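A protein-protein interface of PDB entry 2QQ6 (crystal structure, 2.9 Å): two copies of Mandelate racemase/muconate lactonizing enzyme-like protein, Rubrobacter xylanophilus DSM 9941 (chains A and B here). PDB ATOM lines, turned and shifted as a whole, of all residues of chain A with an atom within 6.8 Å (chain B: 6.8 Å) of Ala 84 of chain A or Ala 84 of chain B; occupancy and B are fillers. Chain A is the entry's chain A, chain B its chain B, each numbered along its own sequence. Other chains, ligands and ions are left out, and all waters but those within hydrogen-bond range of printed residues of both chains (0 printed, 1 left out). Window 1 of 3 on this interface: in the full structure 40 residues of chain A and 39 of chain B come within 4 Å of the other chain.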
ATOM      1  N   ASN A  77     -11.956 -21.372  11.174  1.00  0.00           N
ATOM      2  CA  ASN A  77     -11.320 -20.064  11.028  1.00  0.00           C
ATOM      3  C   ASN A  77     -12.046 -18.958  11.795  1.00  0.00           C
ATOM      4  O   ASN A  77     -11.786 -17.773  11.593  1.00  0.00           O
ATOM      5  CB  ASN A  77     -11.265 -19.697   9.541  1.00  0.00           C
ATOM      6  CG  ASN A  77     -10.298 -20.572   8.746  1.00  0.00           C
ATOM      7  OD1 ASN A  77      -9.101 -20.286   8.685  1.00  0.00           O
ATOM      8  ND2 ASN A  77     -10.815 -21.641   8.134  1.00  0.00           N
ATOM      9  N   THR A  80      -9.677 -16.886  13.319  1.00  0.00           N
ATOM     10  CA  THR A  80      -8.584 -16.546  12.416  1.00  0.00           C
ATOM     11  C   THR A  80      -9.088 -15.925  11.121  1.00  0.00           C
ATOM     12  O   THR A  80      -8.562 -16.223  10.045  1.00  0.00           O
ATOM     13  CB  THR A  80      -7.747 -17.773  12.034  1.00  0.00           C
ATOM     14  OG1 THR A  80      -8.529 -18.647  11.216  1.00  0.00           O
ATOM     15  CG2 THR A  80      -7.291 -18.508  13.268  1.00  0.00           C
ATOM     16  N   GLY A  81     -10.118 -15.083  11.224  1.00  0.00           N
ATOM     17  CA  GLY A  81     -10.658 -14.409  10.051  1.00  0.00           C
ATOM     18  C   GLY A  81     -11.596 -15.203   9.152  1.00  0.00           C
ATOM     19  O   GLY A  81     -11.531 -15.082   7.925  1.00  0.00           O
ATOM     20  N   GLY A  82     -12.472 -16.005   9.752  1.00  0.00           N
ATOM     21  CA  GLY A  82     -13.418 -16.783   8.972  1.00  0.00           C
ATOM     22  C   GLY A  82     -14.682 -16.017   8.610  1.00  0.00           C
ATOM     23  O   GLY A  82     -15.565 -16.530   7.918  1.00  0.00           O
ATOM     24  N   GLN A  83     -14.777 -14.787   9.097  1.00  0.00           N
ATOM     25  CA  GLN A  83     -15.920 -13.929   8.818  1.00  0.00           C
ATOM     26  C   GLN A  83     -15.474 -13.033   7.678  1.00  0.00           C
ATOM     27  O   GLN A  83     -16.256 -12.626   6.811  1.00  0.00           O
ATOM     28  CB  GLN A  83     -16.261 -13.092  10.062  1.00  0.00           C
ATOM     29  CG  GLN A  83     -15.087 -12.797  11.021  1.00  0.00           C
ATOM     30  CD  GLN A  83     -14.787 -13.939  11.997  1.00  0.00           C
ATOM     31  OE1 GLN A  83     -15.695 -14.645  12.434  1.00  0.00           O
ATOM     32  NE2 GLN A  83     -13.510 -14.110  12.354  1.00  0.00           N
ATOM     33  N   ALA A  84     -14.166 -12.792   7.712  1.00  0.00           N
ATOM     34  CA  ALA A  84     -13.369 -11.970   6.794  1.00  0.00           C
ATOM     35  C   ALA A  84     -13.619 -12.029   5.310  1.00  0.00           C
ATOM     36  O   ALA A  84     -14.744 -12.200   4.845  1.00  0.00           O
ATOM     37  CB  ALA A  84     -11.924 -12.268   7.025  1.00  0.00           C
ATOM     38  N   GLY A  85     -12.513 -11.875   4.582  1.00  0.00           N
ATOM     39  CA  GLY A  85     -12.532 -11.882   3.137  1.00  0.00           C
ATOM     40  C   GLY A  85     -11.566 -12.873   2.542  1.00  0.00           C
ATOM     41  O   GLY A  85     -11.987 -13.860   1.966  1.00  0.00           O
ATOM     42  N   ALA A  86     -10.271 -12.626   2.678  1.00  0.00           N
ATOM     43  CA  ALA A  86      -9.272 -13.533   2.116  1.00  0.00           C
ATOM     44  C   ALA A  86      -9.543 -14.974   2.519  1.00  0.00           C
ATOM     45  O   ALA A  86      -9.685 -15.850   1.663  1.00  0.00           O
ATOM     46  CB  ALA A  86      -7.889 -13.127   2.564  1.00  0.00           C
ATOM     47  N   VAL A  87      -9.612 -15.221   3.821  1.00  0.00           N
ATOM     48  CA  VAL A  87      -9.881 -16.560   4.325  1.00  0.00           C
ATOM     49  C   VAL A  87     -11.091 -17.196   3.659  1.00  0.00           C
ATOM     50  O   VAL A  87     -11.152 -18.408   3.501  1.00  0.00           O
ATOM     51  CB  VAL A  87     -10.117 -16.551   5.850  1.00  0.00           C
ATOM     52  CG1 VAL A  87     -10.817 -17.839   6.297  1.00  0.00           C
ATOM     53  CG2 VAL A  87      -8.791 -16.410   6.566  1.00  0.00           C
ATOM     54  N   ILE A  88     -12.061 -16.387   3.269  1.00  0.00           N
ATOM     55  CA  ILE A  88     -13.247 -16.933   2.639  1.00  0.00           C
ATOM     56  C   ILE A  88     -13.087 -17.104   1.131  1.00  0.00           C
ATOM     57  O   ILE A  88     -13.619 -18.044   0.542  1.00  0.00           O
ATOM     58  CB  ILE A  88     -14.462 -16.062   2.959  1.00  0.00           C
ATOM     59  CG1 ILE A  88     -14.763 -16.172   4.454  1.00  0.00           C
ATOM     60  CG2 ILE A  88     -15.653 -16.499   2.139  1.00  0.00           C
ATOM     61  CD1 ILE A  88     -15.801 -15.188   4.958  1.00  0.00           C
ATOM     62  N   THR A  89     -12.348 -16.196   0.509  1.00  0.00           N
ATOM     63  CA  THR A  89     -12.124 -16.286  -0.923  1.00  0.00           C
ATOM     64  C   THR A  89     -11.316 -17.550  -1.136  1.00  0.00           C
ATOM     65  O   THR A  89     -11.523 -18.280  -2.108  1.00  0.00           O
ATOM     66  CB  THR A  89     -11.313 -15.087  -1.463  1.00  0.00           C
ATOM     67  OG1 THR A  89     -12.007 -13.868  -1.178  1.00  0.00           O
ATOM     68  CG2 THR A  89     -11.113 -15.220  -2.973  1.00  0.00           C
ATOM     69  N   TYR A 271     -19.400 -10.634   1.871  1.00  0.00           N
ATOM     70  CA  TYR A 271     -19.033 -12.041   1.851  1.00  0.00           C
ATOM     71  C   TYR A 271     -19.954 -13.188   2.219  1.00  0.00           C
ATOM     72  O   TYR A 271     -20.470 -13.872   1.338  1.00  0.00           O
ATOM     73  CB  TYR A 271     -17.735 -12.218   2.629  1.00  0.00           C
ATOM     74  CG  TYR A 271     -16.542 -11.594   1.946  1.00  0.00           C
ATOM     75  CD1 TYR A 271     -16.304 -10.226   2.029  1.00  0.00           C
ATOM     76  CD2 TYR A 271     -15.653 -12.370   1.210  1.00  0.00           C
ATOM     77  CE1 TYR A 271     -15.211  -9.653   1.405  1.00  0.00           C
ATOM     78  CE2 TYR A 271     -14.567 -11.805   0.585  1.00  0.00           C
ATOM     79  CZ  TYR A 271     -14.348 -10.450   0.691  1.00  0.00           C
ATOM     80  OH  TYR A 271     -13.236  -9.896   0.119  1.00  0.00           O
ATOM     81  N   THR A 272     -20.129 -13.442   3.506  1.00  0.00           N
ATOM     82  CA  THR A 272     -20.953 -14.570   3.906  1.00  0.00           C
ATOM     83  C   THR A 272     -22.435 -14.382   3.633  1.00  0.00           C
ATOM     84  O   THR A 272     -22.880 -13.306   3.246  1.00  0.00           O
ATOM     85  CB  THR A 272     -20.762 -14.896   5.409  1.00  0.00           C
ATOM     86  OG1 THR A 272     -21.121 -13.755   6.197  1.00  0.00           O
ATOM     87  CG2 THR A 272     -19.316 -15.274   5.700  1.00  0.00           C
ATOM     88  N   ASP A 275     -24.084 -11.957   5.899  1.00  0.00           N
ATOM     89  CA  ASP A 275     -23.964 -10.555   5.551  1.00  0.00           C
ATOM     90  C   ASP A 275     -25.025 -10.128   4.555  1.00  0.00           C
ATOM     91  O   ASP A 275     -25.539  -9.021   4.634  1.00  0.00           O
ATOM     92  CB  ASP A 275     -22.571 -10.249   4.996  1.00  0.00           C
ATOM     93  CG  ASP A 275     -21.477 -10.428   6.034  1.00  0.00           C
ATOM     94  OD1 ASP A 275     -21.746 -10.227   7.245  1.00  0.00           O
ATOM     95  OD2 ASP A 275     -20.341 -10.758   5.639  1.00  0.00           O
ATOM     96  N   LYS A 294     -15.406 -15.687  -4.754  1.00  0.00           N
ATOM     97  CA  LYS A 294     -14.912 -14.815  -3.703  1.00  0.00           C
ATOM     98  C   LYS A 294     -15.679 -14.842  -2.385  1.00  0.00           C
ATOM     99  O   LYS A 294     -15.079 -14.644  -1.327  1.00  0.00           O
ATOM    100  CB  LYS A 294     -14.848 -13.381  -4.236  1.00  0.00           C
ATOM    101  CG  LYS A 294     -14.513 -12.320  -3.207  1.00  0.00           C
ATOM    102  CD  LYS A 294     -14.540 -10.921  -3.832  1.00  0.00           C
ATOM    103  CE  LYS A 294     -14.229  -9.836  -2.805  1.00  0.00           C
ATOM    104  NZ  LYS A 294     -14.040  -8.488  -3.413  1.00  0.00           N
ATOM    105  N   GLY B  81     -10.378  -8.037  -0.460  1.00  0.00           N
ATOM    106  CA  GLY B  81     -10.638  -8.537   0.878  1.00  0.00           C
ATOM    107  C   GLY B  81     -10.343  -7.557   1.997  1.00  0.00           C
ATOM    108  O   GLY B  81     -10.087  -7.972   3.126  1.00  0.00           O
ATOM    109  N   GLY B  82     -10.382  -6.264   1.698  1.00  0.00           N
ATOM    110  CA  GLY B  82     -10.116  -5.282   2.723  1.00  0.00           C
ATOM    111  C   GLY B  82     -11.253  -4.968   3.688  1.00  0.00           C
ATOM    112  O   GLY B  82     -11.033  -4.283   4.679  1.00  0.00           O
ATOM    113  N   GLN B  83     -12.459  -5.467   3.437  1.00  0.00           N
ATOM    114  CA  GLN B  83     -13.595  -5.172   4.310  1.00  0.00           C
ATOM    115  C   GLN B  83     -13.371  -5.712   5.701  1.00  0.00           C
ATOM    116  O   GLN B  83     -13.843  -5.117   6.677  1.00  0.00           O
ATOM    117  CB  GLN B  83     -14.900  -5.737   3.753  1.00  0.00           C
ATOM    118  CG  GLN B  83     -14.791  -6.492   2.452  1.00  0.00           C
ATOM    119  CD  GLN B  83     -14.253  -5.637   1.323  1.00  0.00           C
ATOM    120  OE1 GLN B  83     -14.629  -4.485   1.193  1.00  0.00           O
ATOM    121  NE2 GLN B  83     -13.381  -6.206   0.494  1.00  0.00           N
ATOM    122  N   ALA B  84     -12.671  -6.839   5.807  1.00  0.00           N
ATOM    123  CA  ALA B  84     -12.336  -7.403   7.123  1.00  0.00           C
ATOM    124  C   ALA B  84     -11.574  -8.734   7.099  1.00  0.00           C
ATOM    125  O   ALA B  84     -11.361  -9.365   6.057  1.00  0.00           O
ATOM    126  CB  ALA B  84     -13.577  -7.555   7.993  1.00  0.00           C
ATOM    127  N   GLY B  85     -11.157  -9.148   8.289  1.00  0.00           N
ATOM    128  CA  GLY B  85     -10.420 -10.387   8.447  1.00  0.00           C
ATOM    129  C   GLY B  85      -8.913 -10.281   8.320  1.00  0.00           C
ATOM    130  O   GLY B  85      -8.301  -9.325   8.811  1.00  0.00           O
ATOM    131  N   ALA B  86      -8.321 -11.253   7.630  1.00  0.00           N
ATOM    132  CA  ALA B  86      -6.881 -11.303   7.451  1.00  0.00           C
ATOM    133  C   ALA B  86      -6.218  -9.976   7.101  1.00  0.00           C
ATOM    134  O   ALA B  86      -5.431  -9.443   7.887  1.00  0.00           O
ATOM    135  CB  ALA B  86      -6.534 -12.373   6.421  1.00  0.00           C
ATOM    136  N   VAL B  87      -6.543  -9.446   5.928  1.00  0.00           N
ATOM    137  CA  VAL B  87      -5.984  -8.181   5.444  1.00  0.00           C
ATOM    138  C   VAL B  87      -5.990  -7.092   6.506  1.00  0.00           C
ATOM    139  O   VAL B  87      -5.072  -6.286   6.599  1.00  0.00           O
ATOM    140  CB  VAL B  87      -6.778  -7.694   4.232  1.00  0.00           C
ATOM    141  CG1 VAL B  87      -6.226  -6.366   3.716  1.00  0.00           C
ATOM    142  CG2 VAL B  87      -6.728  -8.757   3.155  1.00  0.00           C
ATOM    143  N   ILE B  88      -7.033  -7.086   7.318  1.00  0.00           N
ATOM    144  CA  ILE B  88      -7.169  -6.105   8.387  1.00  0.00           C
ATOM    145  C   ILE B  88      -6.197  -6.386   9.538  1.00  0.00           C
ATOM    146  O   ILE B  88      -5.574  -5.469  10.078  1.00  0.00           O
ATOM    147  CB  ILE B  88      -8.632  -6.075   8.899  1.00  0.00           C
ATOM    148  CG1 ILE B  88      -9.541  -5.468   7.822  1.00  0.00           C
ATOM    149  CG2 ILE B  88      -8.726  -5.285  10.181  1.00  0.00           C
ATOM    150  CD1 ILE B  88      -9.193  -4.037   7.448  1.00  0.00           C
ATOM    151  N   THR B  89      -6.054  -7.656   9.900  1.00  0.00           N
ATOM    152  CA  THR B  89      -5.138  -8.025  10.970  1.00  0.00           C
ATOM    153  C   THR B  89      -3.722  -7.698  10.545  1.00  0.00           C
ATOM    154  O   THR B  89      -2.914  -7.284  11.365  1.00  0.00           O
ATOM    155  CB  THR B  89      -5.195  -9.522  11.293  1.00  0.00           C
ATOM    156  OG1 THR B  89      -6.510  -9.866  11.750  1.00  0.00           O
ATOM    157  CG2 THR B  89      -4.164  -9.863  12.364  1.00  0.00           C
ATOM    158  N   ASN B 269     -14.303 -10.705  17.320  1.00  0.00           N
ATOM    159  CA  ASN B 269     -14.474 -11.215  15.972  1.00  0.00           C
ATOM    160  C   ASN B 269     -15.074 -10.208  14.998  1.00  0.00           C
ATOM    161  O   ASN B 269     -15.445 -10.560  13.885  1.00  0.00           O
ATOM    162  CB  ASN B 269     -15.310 -12.493  15.995  1.00  0.00           C
ATOM    163  CG  ASN B 269     -14.543 -13.669  16.549  1.00  0.00           C
ATOM    164  OD1 ASN B 269     -13.413 -13.931  16.138  1.00  0.00           O
ATOM    165  ND2 ASN B 269     -15.151 -14.390  17.484  1.00  0.00           N
ATOM    166  N   VAL B 270     -15.160  -8.951  15.413  1.00  0.00           N
ATOM    167  CA  VAL B 270     -15.688  -7.911  14.545  1.00  0.00           C
ATOM    168  C   VAL B 270     -14.552  -6.933  14.245  1.00  0.00           C
ATOM    169  O   VAL B 270     -13.834  -6.524  15.157  1.00  0.00           O
ATOM    170  CB  VAL B 270     -16.883  -7.189  15.218  1.00  0.00           C
ATOM    171  CG1 VAL B 270     -16.609  -6.992  16.694  1.00  0.00           C
ATOM    172  CG2 VAL B 270     -17.135  -5.851  14.550  1.00  0.00           C
ATOM    173  N   TYR B 271     -14.376  -6.580  12.971  1.00  0.00           N
ATOM    174  CA  TYR B 271     -13.304  -5.664  12.573  1.00  0.00           C
ATOM    175  C   TYR B 271     -13.832  -4.315  12.094  1.00  0.00           C
ATOM    176  O   TYR B 271     -14.959  -4.221  11.619  1.00  0.00           O
ATOM    177  CB  TYR B 271     -12.485  -6.255  11.422  1.00  0.00           C
ATOM    178  CG  TYR B 271     -12.074  -7.702  11.546  1.00  0.00           C
ATOM    179  CD1 TYR B 271     -13.023  -8.716  11.599  1.00  0.00           C
ATOM    180  CD2 TYR B 271     -10.721  -8.061  11.569  1.00  0.00           C
ATOM    181  CE1 TYR B 271     -12.637 -10.055  11.669  1.00  0.00           C
ATOM    182  CE2 TYR B 271     -10.324  -9.395  11.639  1.00  0.00           C
ATOM    183  CZ  TYR B 271     -11.287 -10.387  11.687  1.00  0.00           C
ATOM    184  OH  TYR B 271     -10.910 -11.712  11.738  1.00  0.00           O
ATOM    185  N   THR B 272     -13.000  -3.282  12.201  1.00  0.00           N
ATOM    186  CA  THR B 272     -13.319  -1.912  11.746  1.00  0.00           C
ATOM    187  C   THR B 272     -14.445  -1.150  12.412  1.00  0.00           C
ATOM    188  O   THR B 272     -15.443  -1.713  12.865  1.00  0.00           O
ATOM    189  CB  THR B 272     -13.609  -1.817  10.211  1.00  0.00           C
ATOM    190  OG1 THR B 272     -14.833  -2.489   9.901  1.00  0.00           O
ATOM    191  CG2 THR B 272     -12.477  -2.415   9.407  1.00  0.00           C
ATOM    192  N   ASP B 275     -18.066  -1.774  11.499  1.00  0.00           N
ATOM    193  CA  ASP B 275     -18.778  -2.904  12.053  1.00  0.00           C
ATOM    194  C   ASP B 275     -19.145  -2.735  13.518  1.00  0.00           C
ATOM    195  O   ASP B 275     -20.153  -3.262  13.975  1.00  0.00           O
ATOM    196  CB  ASP B 275     -17.972  -4.175  11.836  1.00  0.00           C
ATOM    197  CG  ASP B 275     -17.797  -4.498  10.364  1.00  0.00           C
ATOM    198  OD1 ASP B 275     -18.813  -4.646   9.651  1.00  0.00           O
ATOM    199  OD2 ASP B 275     -16.639  -4.602   9.916  1.00  0.00           O
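Gly 81 of chain A touches Tyr 271 of chain B, and with the chains exchanged Tyr 271 of chain A touches Gly 81 of chain B.
Gln 83 of chain A touches Tyr 271 of chain B, and with the chains exchanged Tyr 271 of chain A touches Gln 83 of chain B.
Ala 84 of chain B touches its own counterpart, Ala 84 of chain A.
Ala 84 of chain A touches Gly 85 of chain B, and with the chains exchanged Gly 85 of chain A touches Ala 84 of chain B.
Of the 9 pairs that touch across the chains among the printed residues, 7 have their exchanged pair printed and touching as well.
OH of Tyr 271 of chain B touches CA of Gly 81 of chain A (3.2 Å).
Gln 83 of chain A touches Asn 269 of chain B (CG to O, 3.7 Å).
OH of Tyr 271 of chain B touches NE2 of Gln 83 of chain A, at 3.6 Å.
CB of Ala 84 of chain A touches O of Ala 84 of chain B, 3.1 Å away.
Ala 84 of chain A touches Gly 85 of chain B.
CB of Ala 84 of chain A touches N of Ala 86 of chain B, at 3.8 Å.
Tyr 271 of chain A touches Gln 83 of chain B (CE1 to CG, 3.4 Å).
Hydrophobic or aromatic side chains of chain B that line the printed part of chain A: Tyr 271.
Of the 15 printed residues of chain A, 5 touch a printed residue of chain B.
Printed residues of chain A that touch a printed residue of chain B: Gly 81, Gln 83, Ala 84, Gly 85 and Tyr 271.
Hydrophobic or aromatic side chains of chain A that line the printed part of chain B: Ala 84 and Tyr 271.
Among the printed residues, 9 pairs touch across the chains.
Among the printed residues, no Asp or Glu carboxylate lies within 4 Å of a Lys or Arg side-chain nitrogen of the other chain.
The backbone NH (N) of Gly 85 of chain A lies within hydrogen-bond range of the backbone carbonyl oxygen (O) of Ala 84 of chain B.
The backbone NH of Gly 81 of chain B sits close to the side-chain hydroxyl of Tyr 271 of chain A, at 3.5 Å.
O of Gly 85 of chain A sits at hydrogen-bond distance from OG1 of Thr 89 of chain A.
The side-chain carboxylate (OD2) of Asp 275 of chain B sits close to the backbone carbonyl oxygen (O) of Tyr 271 of chain B (2.4 Å).
The backbone carbonyl oxygen of Gly 85 of chain B sits at hydrogen-bond distance from the side-chain hydroxyl of Thr 89 of chain B, 3.5 Å away.
Printed residues of chain A within 4 Å of Ala 84 of chain B: Ala 84 and Gly 85.
Of the printed residues of chain A, Tyr 271 of chain B touches Gly 81 and Gln 83.
Printed residues of chain A within 4 Å of Gly 85 of chain B: Ala 84.
Of the printed residues of chain B, Gln 83 of chain A touches Asn 269 and Tyr 271.
Of the printed residues of chain A, Gly 81 of chain B touches Tyr 271.
Of the printed residues of chain B, Gly 85 of chain A touches Ala 84.
Asn 77 of chain A touches none of the printed residues of chain B.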
